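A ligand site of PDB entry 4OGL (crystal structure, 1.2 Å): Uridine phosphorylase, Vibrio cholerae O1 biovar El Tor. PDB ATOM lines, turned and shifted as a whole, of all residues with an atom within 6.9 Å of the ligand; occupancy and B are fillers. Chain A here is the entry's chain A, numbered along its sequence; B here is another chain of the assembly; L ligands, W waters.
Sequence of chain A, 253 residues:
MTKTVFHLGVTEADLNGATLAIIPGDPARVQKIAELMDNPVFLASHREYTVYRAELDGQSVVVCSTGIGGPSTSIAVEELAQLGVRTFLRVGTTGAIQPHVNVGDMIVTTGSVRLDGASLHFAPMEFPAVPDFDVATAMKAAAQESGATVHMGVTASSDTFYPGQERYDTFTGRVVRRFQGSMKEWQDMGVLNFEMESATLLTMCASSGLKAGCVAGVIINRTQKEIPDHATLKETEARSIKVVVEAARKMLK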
ATOM      1  N   GLY A  92       4.069  20.783  -8.195  1.00  0.00           N
ATOM      2  CA  GLY A  92       3.848  21.911  -7.315  1.00  0.00           C
ATOM      3  C   GLY A  92       3.783  21.487  -5.867  1.00  0.00           C
ATOM      4  O   GLY A  92       4.031  20.334  -5.558  1.00  0.00           O
ATOM      5  N   THR A  93       3.463  22.445  -4.990  1.00  0.00           N
ATOM      6  CA  THR A  93       3.257  22.183  -3.581  1.00  0.00           C
ATOM      7  C   THR A  93       1.785  22.146  -3.286  1.00  0.00           C
ATOM      8  O   THR A  93       0.951  22.618  -4.063  1.00  0.00           O
ATOM      9  CB  THR A  93       3.877  23.298  -2.688  1.00  0.00           C
ATOM     10  OG1 THR A  93       3.278  24.563  -3.012  1.00  0.00           O
ATOM     11  CG2 THR A  93       5.381  23.371  -2.893  1.00  0.00           C
ATOM     12  N   THR A  94       1.450  21.573  -2.146  1.00  0.00           N
ATOM     13  CA  THR A  94       0.060  21.404  -1.808  1.00  0.00           C
ATOM     14  C   THR A  94      -0.163  21.368  -0.300  1.00  0.00           C
ATOM     15  O   THR A  94       0.751  21.087   0.461  1.00  0.00           O
ATOM     16  CB  THR A  94      -0.495  20.141  -2.499  1.00  0.00           C
ATOM     17  OG1 THR A  94      -1.910  20.099  -2.346  1.00  0.00           O
ATOM     18  CG2 THR A  94       0.062  18.877  -1.913  1.00  0.00           C
ATOM     19  N   GLY A  95      -1.390  21.666   0.110  1.00  0.00           N
ATOM     20  CA  GLY A  95      -1.807  21.496   1.488  1.00  0.00           C
ATOM     21  C   GLY A  95      -2.697  20.274   1.571  1.00  0.00           C
ATOM     22  O   GLY A  95      -3.719  20.202   0.899  1.00  0.00           O
ATOM     23  N   ALA A  96      -2.341  19.330   2.435  1.00  0.00           N
ATOM     24  CA  ALA A  96      -3.157  18.144   2.626  1.00  0.00           C
ATOM     25  C   ALA A  96      -4.308  18.443   3.545  1.00  0.00           C
ATOM     26  O   ALA A  96      -4.188  19.259   4.463  1.00  0.00           O
ATOM     27  CB  ALA A  96      -2.310  17.029   3.208  1.00  0.00           C
ATOM     28  N   ALA A 156      -8.832  19.027  -4.440  1.00  0.00           N
ATOM     29  CA  ALA A 156      -9.715  20.176  -4.589  1.00  0.00           C
ATOM     30  C   ALA A 156      -8.921  21.346  -5.161  1.00  0.00           C
ATOM     31  O   ALA A 156      -7.921  21.752  -4.576  1.00  0.00           O
ATOM     32  CB  ALA A 156     -10.343  20.548  -3.254  1.00  0.00           C
ATOM     33  N   SER A 158      -8.743  25.104  -6.386  1.00  0.00           N
ATOM     34  CA  SER A 158      -9.421  26.355  -6.057  1.00  0.00           C
ATOM     35  C   SER A 158      -8.861  27.581  -6.770  1.00  0.00           C
ATOM     36  O   SER A 158      -7.643  27.761  -6.861  1.00  0.00           O
ATOM     37  CB  SER A 158      -9.293  26.548  -4.542  1.00  0.00           C
ATOM     38  OG  SER A 158      -9.798  27.815  -4.138  1.00  0.00           O
ATOM     39  N   THR A 160      -8.906  30.425  -5.479  1.00  0.00           N
ATOM     40  CA  THR A 160      -8.272  31.286  -4.476  1.00  0.00           C
ATOM     41  C   THR A 160      -7.423  30.447  -3.523  1.00  0.00           C
ATOM     42  O   THR A 160      -7.659  29.249  -3.330  1.00  0.00           O
ATOM     43  CB  THR A 160      -9.306  32.108  -3.661  1.00  0.00           C
ATOM     44  OG1 THR A 160     -10.217  31.215  -2.995  1.00  0.00           O
ATOM     45  CG2 THR A 160     -10.063  33.066  -4.572  1.00  0.00           C
ATOM     46  N   PHE A 161      -6.472  31.091  -2.888  1.00  0.00           N
ATOM     47  CA  PHE A 161      -5.669  30.478  -1.835  1.00  0.00           C
ATOM     48  C   PHE A 161      -6.387  30.590  -0.496  1.00  0.00           C
ATOM     49  O   PHE A 161      -6.210  29.756   0.388  1.00  0.00           O
ATOM     50  CB  PHE A 161      -4.315  31.173  -1.781  1.00  0.00           C
ATOM     51  CG  PHE A 161      -3.336  30.554  -0.824  1.00  0.00           C
ATOM     52  CD1 PHE A 161      -2.549  29.465  -1.201  1.00  0.00           C
ATOM     53  CD2 PHE A 161      -3.175  31.076   0.442  1.00  0.00           C
ATOM     54  CE1 PHE A 161      -1.612  28.918  -0.320  1.00  0.00           C
ATOM     55  CE2 PHE A 161      -2.237  30.540   1.323  1.00  0.00           C
ATOM     56  CZ  PHE A 161      -1.471  29.461   0.948  1.00  0.00           C
ATOM     57  N   GLN A 165     -10.077  27.850   0.007  1.00  0.00           N
ATOM     58  CA  GLN A 165      -9.445  26.788   0.768  1.00  0.00           C
ATOM     59  C   GLN A 165      -9.848  26.934   2.238  1.00  0.00           C
ATOM     60  O   GLN A 165      -9.211  26.369   3.118  1.00  0.00           O
ATOM     61  CB  GLN A 165      -7.920  26.791   0.570  1.00  0.00           C
ATOM     62  CG  GLN A 165      -7.597  26.716  -0.905  1.00  0.00           C
ATOM     63  CD  GLN A 165      -6.126  26.513  -1.209  1.00  0.00           C
ATOM     64  OE1 GLN A 165      -5.371  25.960  -0.403  1.00  0.00           O
ATOM     65  NE2 GLN A 165      -5.713  26.927  -2.398  1.00  0.00           N
ATOM     66  N   ARG A 167      -9.624  29.302   4.443  1.00  0.00           N
ATOM     67  CA  ARG A 167      -8.753  29.974   5.402  1.00  0.00           C
ATOM     68  C   ARG A 167      -9.471  31.163   6.030  1.00  0.00           C
ATOM     69  O   ARG A 167     -10.132  31.932   5.329  1.00  0.00           O
ATOM     70  CB  ARG A 167      -7.483  30.437   4.699  1.00  0.00           C
ATOM     71  CG  ARG A 167      -6.515  29.306   4.375  1.00  0.00           C
ATOM     72  CD  ARG A 167      -5.224  29.827   3.723  1.00  0.00           C
ATOM     73  NE  ARG A 167      -4.162  28.819   3.832  1.00  0.00           N
ATOM     74  CZ  ARG A 167      -3.882  27.902   2.917  1.00  0.00           C
ATOM     75  NH1 ARG A 167      -4.539  27.888   1.756  1.00  0.00           N
ATOM     76  NH2 ARG A 167      -2.945  27.000   3.164  1.00  0.00           N
ATOM     77  N   PHE A 194      -5.509  20.461  -1.327  1.00  0.00           N
ATOM     78  CA  PHE A 194      -5.871  21.671  -2.061  1.00  0.00           C
ATOM     79  C   PHE A 194      -4.696  22.130  -2.912  1.00  0.00           C
ATOM     80  O   PHE A 194      -3.551  22.159  -2.446  1.00  0.00           O
ATOM     81  CB  PHE A 194      -6.139  22.857  -1.107  1.00  0.00           C
ATOM     82  CG  PHE A 194      -7.509  22.886  -0.452  1.00  0.00           C
ATOM     83  CD1 PHE A 194      -8.662  23.087  -1.189  1.00  0.00           C
ATOM     84  CD2 PHE A 194      -7.615  22.834   0.941  1.00  0.00           C
ATOM     85  CE1 PHE A 194      -9.912  23.176  -0.535  1.00  0.00           C
ATOM     86  CE2 PHE A 194      -8.845  22.933   1.575  1.00  0.00           C
ATOM     87  CZ  PHE A 194      -9.989  23.094   0.846  1.00  0.00           C
ATOM     88  N   GLU A 195      -4.984  22.587  -4.117  1.00  0.00           N
ATOM     89  CA  GLU A 195      -4.057  23.424  -4.896  1.00  0.00           C
ATOM     90  C   GLU A 195      -4.885  24.292  -5.828  1.00  0.00           C
ATOM     91  O   GLU A 195      -6.099  24.387  -5.616  1.00  0.00           O
ATOM     92  CB  GLU A 195      -2.939  22.616  -5.572  1.00  0.00           C
ATOM     93  CG  GLU A 195      -3.427  21.467  -6.401  1.00  0.00           C
ATOM     94  CD  GLU A 195      -4.037  21.918  -7.686  1.00  0.00           C
ATOM     95  OE1 GLU A 195      -5.271  21.905  -7.788  1.00  0.00           O
ATOM     96  OE2 GLU A 195      -3.285  22.330  -8.596  1.00  0.00           O
ATOM     97  N   MET A 196      -4.265  24.948  -6.814  1.00  0.00           N
ATOM     98  CA  MET A 196      -4.967  25.998  -7.553  1.00  0.00           C
ATOM     99  C   MET A 196      -4.945  25.875  -9.070  1.00  0.00           C
ATOM    100  O   MET A 196      -5.455  26.763  -9.741  1.00  0.00           O
ATOM    101  CB  MET A 196      -4.403  27.374  -7.188  1.00  0.00           C
ATOM    102  CG  MET A 196      -4.595  27.669  -5.699  1.00  0.00           C
ATOM    103  SD  MET A 196      -4.006  29.268  -5.177  1.00  0.00           S
ATOM    104  CE  MET A 196      -5.036  30.350  -6.175  1.00  0.00           C
ATOM    105  N   GLU A 197      -4.364  24.824  -9.629  1.00  0.00           N
ATOM    106  CA  GLU A 197      -4.231  24.769 -11.097  1.00  0.00           C
ATOM    107  C   GLU A 197      -4.734  23.504 -11.749  1.00  0.00           C
ATOM    108  O   GLU A 197      -5.002  23.500 -12.953  1.00  0.00           O
ATOM    109  CB  GLU A 197      -2.773  25.001 -11.525  1.00  0.00           C
ATOM    110  CG  GLU A 197      -2.220  26.388 -11.209  1.00  0.00           C
ATOM    111  CD  GLU A 197      -1.764  26.533  -9.766  1.00  0.00           C
ATOM    112  OE1 GLU A 197      -1.485  25.516  -9.093  1.00  0.00           O
ATOM    113  OE2 GLU A 197      -1.658  27.686  -9.306  1.00  0.00           O
ATOM    114  N   GLY A 217       4.042  17.876  -3.819  1.00  0.00           N
ATOM    115  CA  GLY A 217       4.613  17.605  -2.516  1.00  0.00           C
ATOM    116  C   GLY A 217       3.848  18.327  -1.433  1.00  0.00           C
ATOM    117  O   GLY A 217       3.536  19.513  -1.548  1.00  0.00           O
ATOM    118  N   VAL A 218       3.541  17.607  -0.359  1.00  0.00           N
ATOM    119  CA  VAL A 218       2.746  18.159   0.738  1.00  0.00           C
ATOM    120  C   VAL A 218       3.657  18.983   1.642  1.00  0.00           C
ATOM    121  O   VAL A 218       4.624  18.458   2.202  1.00  0.00           O
ATOM    122  CB  VAL A 218       2.090  17.018   1.567  1.00  0.00           C
ATOM    123  CG1 VAL A 218       1.359  17.575   2.782  1.00  0.00           C
ATOM    124  CG2 VAL A 218       1.130  16.214   0.686  1.00  0.00           C
ATOM    125  N   ILE A 219       3.333  20.259   1.790  1.00  0.00           N
ATOM    126  CA  ILE A 219       4.142  21.114   2.658  1.00  0.00           C
ATOM    127  C   ILE A 219       3.422  21.590   3.910  1.00  0.00           C
ATOM    128  O   ILE A 219       4.021  22.237   4.757  1.00  0.00           O
ATOM    129  CB  ILE A 219       4.771  22.302   1.902  1.00  0.00           C
ATOM    130  CG1 ILE A 219       3.694  23.256   1.351  1.00  0.00           C
ATOM    131  CG2 ILE A 219       5.645  21.782   0.773  1.00  0.00           C
ATOM    132  CD1 ILE A 219       4.282  24.583   0.892  1.00  0.00           C
ATOM    133  N   ILE A 220       2.135  21.279   4.019  1.00  0.00           N
ATOM    134  CA  ILE A 220       1.362  21.597   5.207  1.00  0.00           C
ATOM    135  C   ILE A 220       0.223  20.606   5.286  1.00  0.00           C
ATOM    136  O   ILE A 220      -0.271  20.146   4.253  1.00  0.00           O
ATOM    137  CB  ILE A 220       0.804  23.060   5.180  1.00  0.00           C
ATOM    138  CG1 ILE A 220       0.065  23.434   6.469  1.00  0.00           C
ATOM    139  CG2 ILE A 220      -0.104  23.278   3.985  1.00  0.00           C
ATOM    140  CD1 ILE A 220      -0.342  24.905   6.507  1.00  0.00           C
ATOM    141  N   ARG A 222      -3.525  20.775   6.662  1.00  0.00           N
ATOM    142  CA  ARG A 222      -4.530  21.752   7.111  1.00  0.00           C
ATOM    143  C   ARG A 222      -5.312  21.317   8.351  1.00  0.00           C
ATOM    144  O   ARG A 222      -6.032  22.127   8.945  1.00  0.00           O
ATOM    145  CB  ARG A 222      -5.486  22.068   5.962  1.00  0.00           C
ATOM    146  CG  ARG A 222      -4.850  22.879   4.831  1.00  0.00           C
ATOM    147  CD  ARG A 222      -4.474  24.323   5.264  1.00  0.00           C
ATOM    148  NE  ARG A 222      -5.636  25.005   5.837  1.00  0.00           N
ATOM    149  CZ  ARG A 222      -6.648  25.476   5.116  1.00  0.00           C
ATOM    150  NH1 ARG A 222      -6.620  25.436   3.782  1.00  0.00           N
ATOM    151  NH2 ARG A 222      -7.699  26.026   5.720  1.00  0.00           N
ATOM    152  N   GLU A 226      -3.062  26.709   9.304  1.00  0.00           N
ATOM    153  CA  GLU A 226      -3.432  27.309   8.017  1.00  0.00           C
ATOM    154  C   GLU A 226      -2.280  27.680   7.094  1.00  0.00           C
ATOM    155  O   GLU A 226      -2.428  27.627   5.875  1.00  0.00           O
ATOM    156  CB  GLU A 226      -4.264  28.575   8.201  1.00  0.00           C
ATOM    157  CG  GLU A 226      -5.704  28.305   8.567  1.00  0.00           C
ATOM    158  CD  GLU A 226      -6.626  29.533   8.462  1.00  0.00           C
ATOM    159  OE1 GLU A 226      -6.198  30.629   8.009  1.00  0.00           O
ATOM    160  OE2 GLU A 226      -7.814  29.391   8.855  1.00  0.00           O
ATOM    161  N   PRO A 228       1.936  27.572   5.945  1.00  0.00           N
ATOM    162  CA  PRO A 228       3.231  26.901   6.109  1.00  0.00           C
ATOM    163  C   PRO A 228       4.272  27.825   6.732  1.00  0.00           C
ATOM    164  O   PRO A 228       4.227  29.045   6.509  1.00  0.00           O
ATOM    165  CB  PRO A 228       3.645  26.544   4.671  1.00  0.00           C
ATOM    166  CG  PRO A 228       2.399  26.607   3.882  1.00  0.00           C
ATOM    167  CD  PRO A 228       1.561  27.656   4.518  1.00  0.00           C
ATOM    168  N   PHE B   6       2.662  35.419   3.185  1.00  0.00           N
ATOM    169  CA  PHE B   6       3.204  34.166   2.660  1.00  0.00           C
ATOM    170  C   PHE B   6       3.729  34.239   1.224  1.00  0.00           C
ATOM    171  O   PHE B   6       4.798  33.717   0.911  1.00  0.00           O
ATOM    172  CB  PHE B   6       2.176  33.043   2.810  1.00  0.00           C
ATOM    173  CG  PHE B   6       2.671  31.706   2.384  1.00  0.00           C
ATOM    174  CD1 PHE B   6       3.682  31.067   3.088  1.00  0.00           C
ATOM    175  CD2 PHE B   6       2.134  31.069   1.275  1.00  0.00           C
ATOM    176  CE1 PHE B   6       4.158  29.829   2.686  1.00  0.00           C
ATOM    177  CE2 PHE B   6       2.599  29.833   0.863  1.00  0.00           C
ATOM    178  CZ  PHE B   6       3.611  29.213   1.569  1.00  0.00           C
ATOM    179  N   HIS B   7       2.972  34.884   0.352  1.00  0.00           N
ATOM    180  CA  HIS B   7       3.388  34.986  -1.049  1.00  0.00           C
ATOM    181  C   HIS B   7       4.191  36.236  -1.358  1.00  0.00           C
ATOM    182  O   HIS B   7       5.178  36.160  -2.073  1.00  0.00           O
ATOM    183  CB  HIS B   7       2.187  34.925  -1.995  1.00  0.00           C
ATOM    184  CG  HIS B   7       1.466  33.615  -1.962  1.00  0.00           C
ATOM    185  ND1 HIS B   7       0.432  33.375  -1.097  1.00  0.00           N
ATOM    186  CD2 HIS B   7       1.631  32.481  -2.701  1.00  0.00           C
ATOM    187  CE1 HIS B   7      -0.026  32.143  -1.299  1.00  0.00           C
ATOM    188  NE2 HIS B   7       0.693  31.587  -2.254  1.00  0.00           N
ATOM    189  N   ARG B  47       7.764  34.877  -7.239  1.00  0.00           N
ATOM    190  CA  ARG B  47       6.801  34.457  -8.256  1.00  0.00           C
ATOM    191  C   ARG B  47       6.455  35.672  -9.130  1.00  0.00           C
ATOM    192  O   ARG B  47       7.346  36.443  -9.479  1.00  0.00           O
ATOM    193  CB  ARG B  47       5.570  33.836  -7.600  1.00  0.00           C
ATOM    194  CG  ARG B  47       5.861  32.526  -6.867  1.00  0.00           C
ATOM    195  CD  ARG B  47       4.556  31.960  -6.337  1.00  0.00           C
ATOM    196  NE  ARG B  47       4.674  30.645  -5.719  1.00  0.00           N
ATOM    197  CZ  ARG B  47       4.284  29.507  -6.281  1.00  0.00           C
ATOM    198  NH1 ARG B  47       3.755  29.484  -7.496  1.00  0.00           N
ATOM    199  NH2 ARG B  47       4.433  28.370  -5.607  1.00  0.00           N
HETATM  200  N1  LIG L   1      -0.889  25.600  -2.591  1.00  0.00           N
HETATM  201  C1  LIG L   1      -2.260  25.713  -2.303  1.00  0.00           C
HETATM  202  O1  LIG L   1      -3.057  25.998  -3.168  1.00  0.00           O
HETATM  203  N2  LIG L   1      -2.679  25.504  -0.986  1.00  0.00           N
HETATM  204  C2  LIG L   1      -1.786  25.223   0.047  1.00  0.00           C
HETATM  205  O2  LIG L   1      -2.211  25.071   1.186  1.00  0.00           O
HETATM  206  C3  LIG L   1      -0.356  25.120  -0.273  1.00  0.00           C
HETATM  207  C4  LIG L   1       0.637  24.808   0.776  1.00  0.00           C
HETATM  208  C5  LIG L   1       0.064  25.298  -1.571  1.00  0.00           C
HETATM  209  O   HOH W   1      -4.803  24.374   1.822  1.00  0.00           O
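OE1 of Gln 165 is in hydrogen-bond range of N2 of the ligand (2.8 Å).
NH2 of Arg 167 lies within hydrogen-bond range of O2 of the ligand (2.9 Å).
Water W1 lies within hydrogen-bond range of an oxygen (O2) of the ligand, the side-chain amide oxygen of Gln 165, the guanidinium group of Arg 222 and the guanidinium group of Arg 167.
Merely in contact with the ligand: Thr 93 (3.6 Å), Thr 94 (3.7 Å), Gly 95 (3.6 Å), Phe 161 (3.6 Å), Phe 194 (3.8 Å), Glu 195 (3.3 Å), Met 196 (3.4 Å), Ile 219 (3.5 Å), Ile 220 (3.6 Å) and Pro 228 (3.999 Å).
Hydrophobic or aromatic side chains that line the ligand: Phe 161, Met 196, Ile 219, Ile 220 and Pro 228.
Within 4 Å of the ligand: Thr 93, Thr 94, Gly 95, Phe 161, Gln 165, Arg 167, Phe 194, Glu 195, Met 196, Ile 219, Ile 220 and Pro 228.
Along chain A the residues within 4 Å of the ligand span positions 93 to 228.
The side-chain amide oxygen of Gln 165 lies within hydrogen-bond range of the guanidinium group of Arg 167 (3.0 Å).
The side-chain amide nitrogen (NE2) of Gln 165 is in hydrogen-bond range of the backbone carbonyl oxygen (O) of Thr 160 (3.2 Å).
The guanidinium group of Arg 167 sits at hydrogen-bond distance from the backbone carbonyl oxygen of Phe 161 (2.9 Å).
O of Glu 226 is in hydrogen-bond range of NH2 of Arg 167.
The side-chain carboxylate of Glu 195 is in hydrogen-bond range of the backbone NH of Glu 197.
N of Glu 195 lies within hydrogen-bond range of O of Ala 156 (3.1 Å).
N of Ile 219 lies within hydrogen-bond range of O of Thr 94 (3.0 Å).
The backbone NH (N) of Thr 94 sits at hydrogen-bond distance from the backbone carbonyl oxygen (O) of Gly 217.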
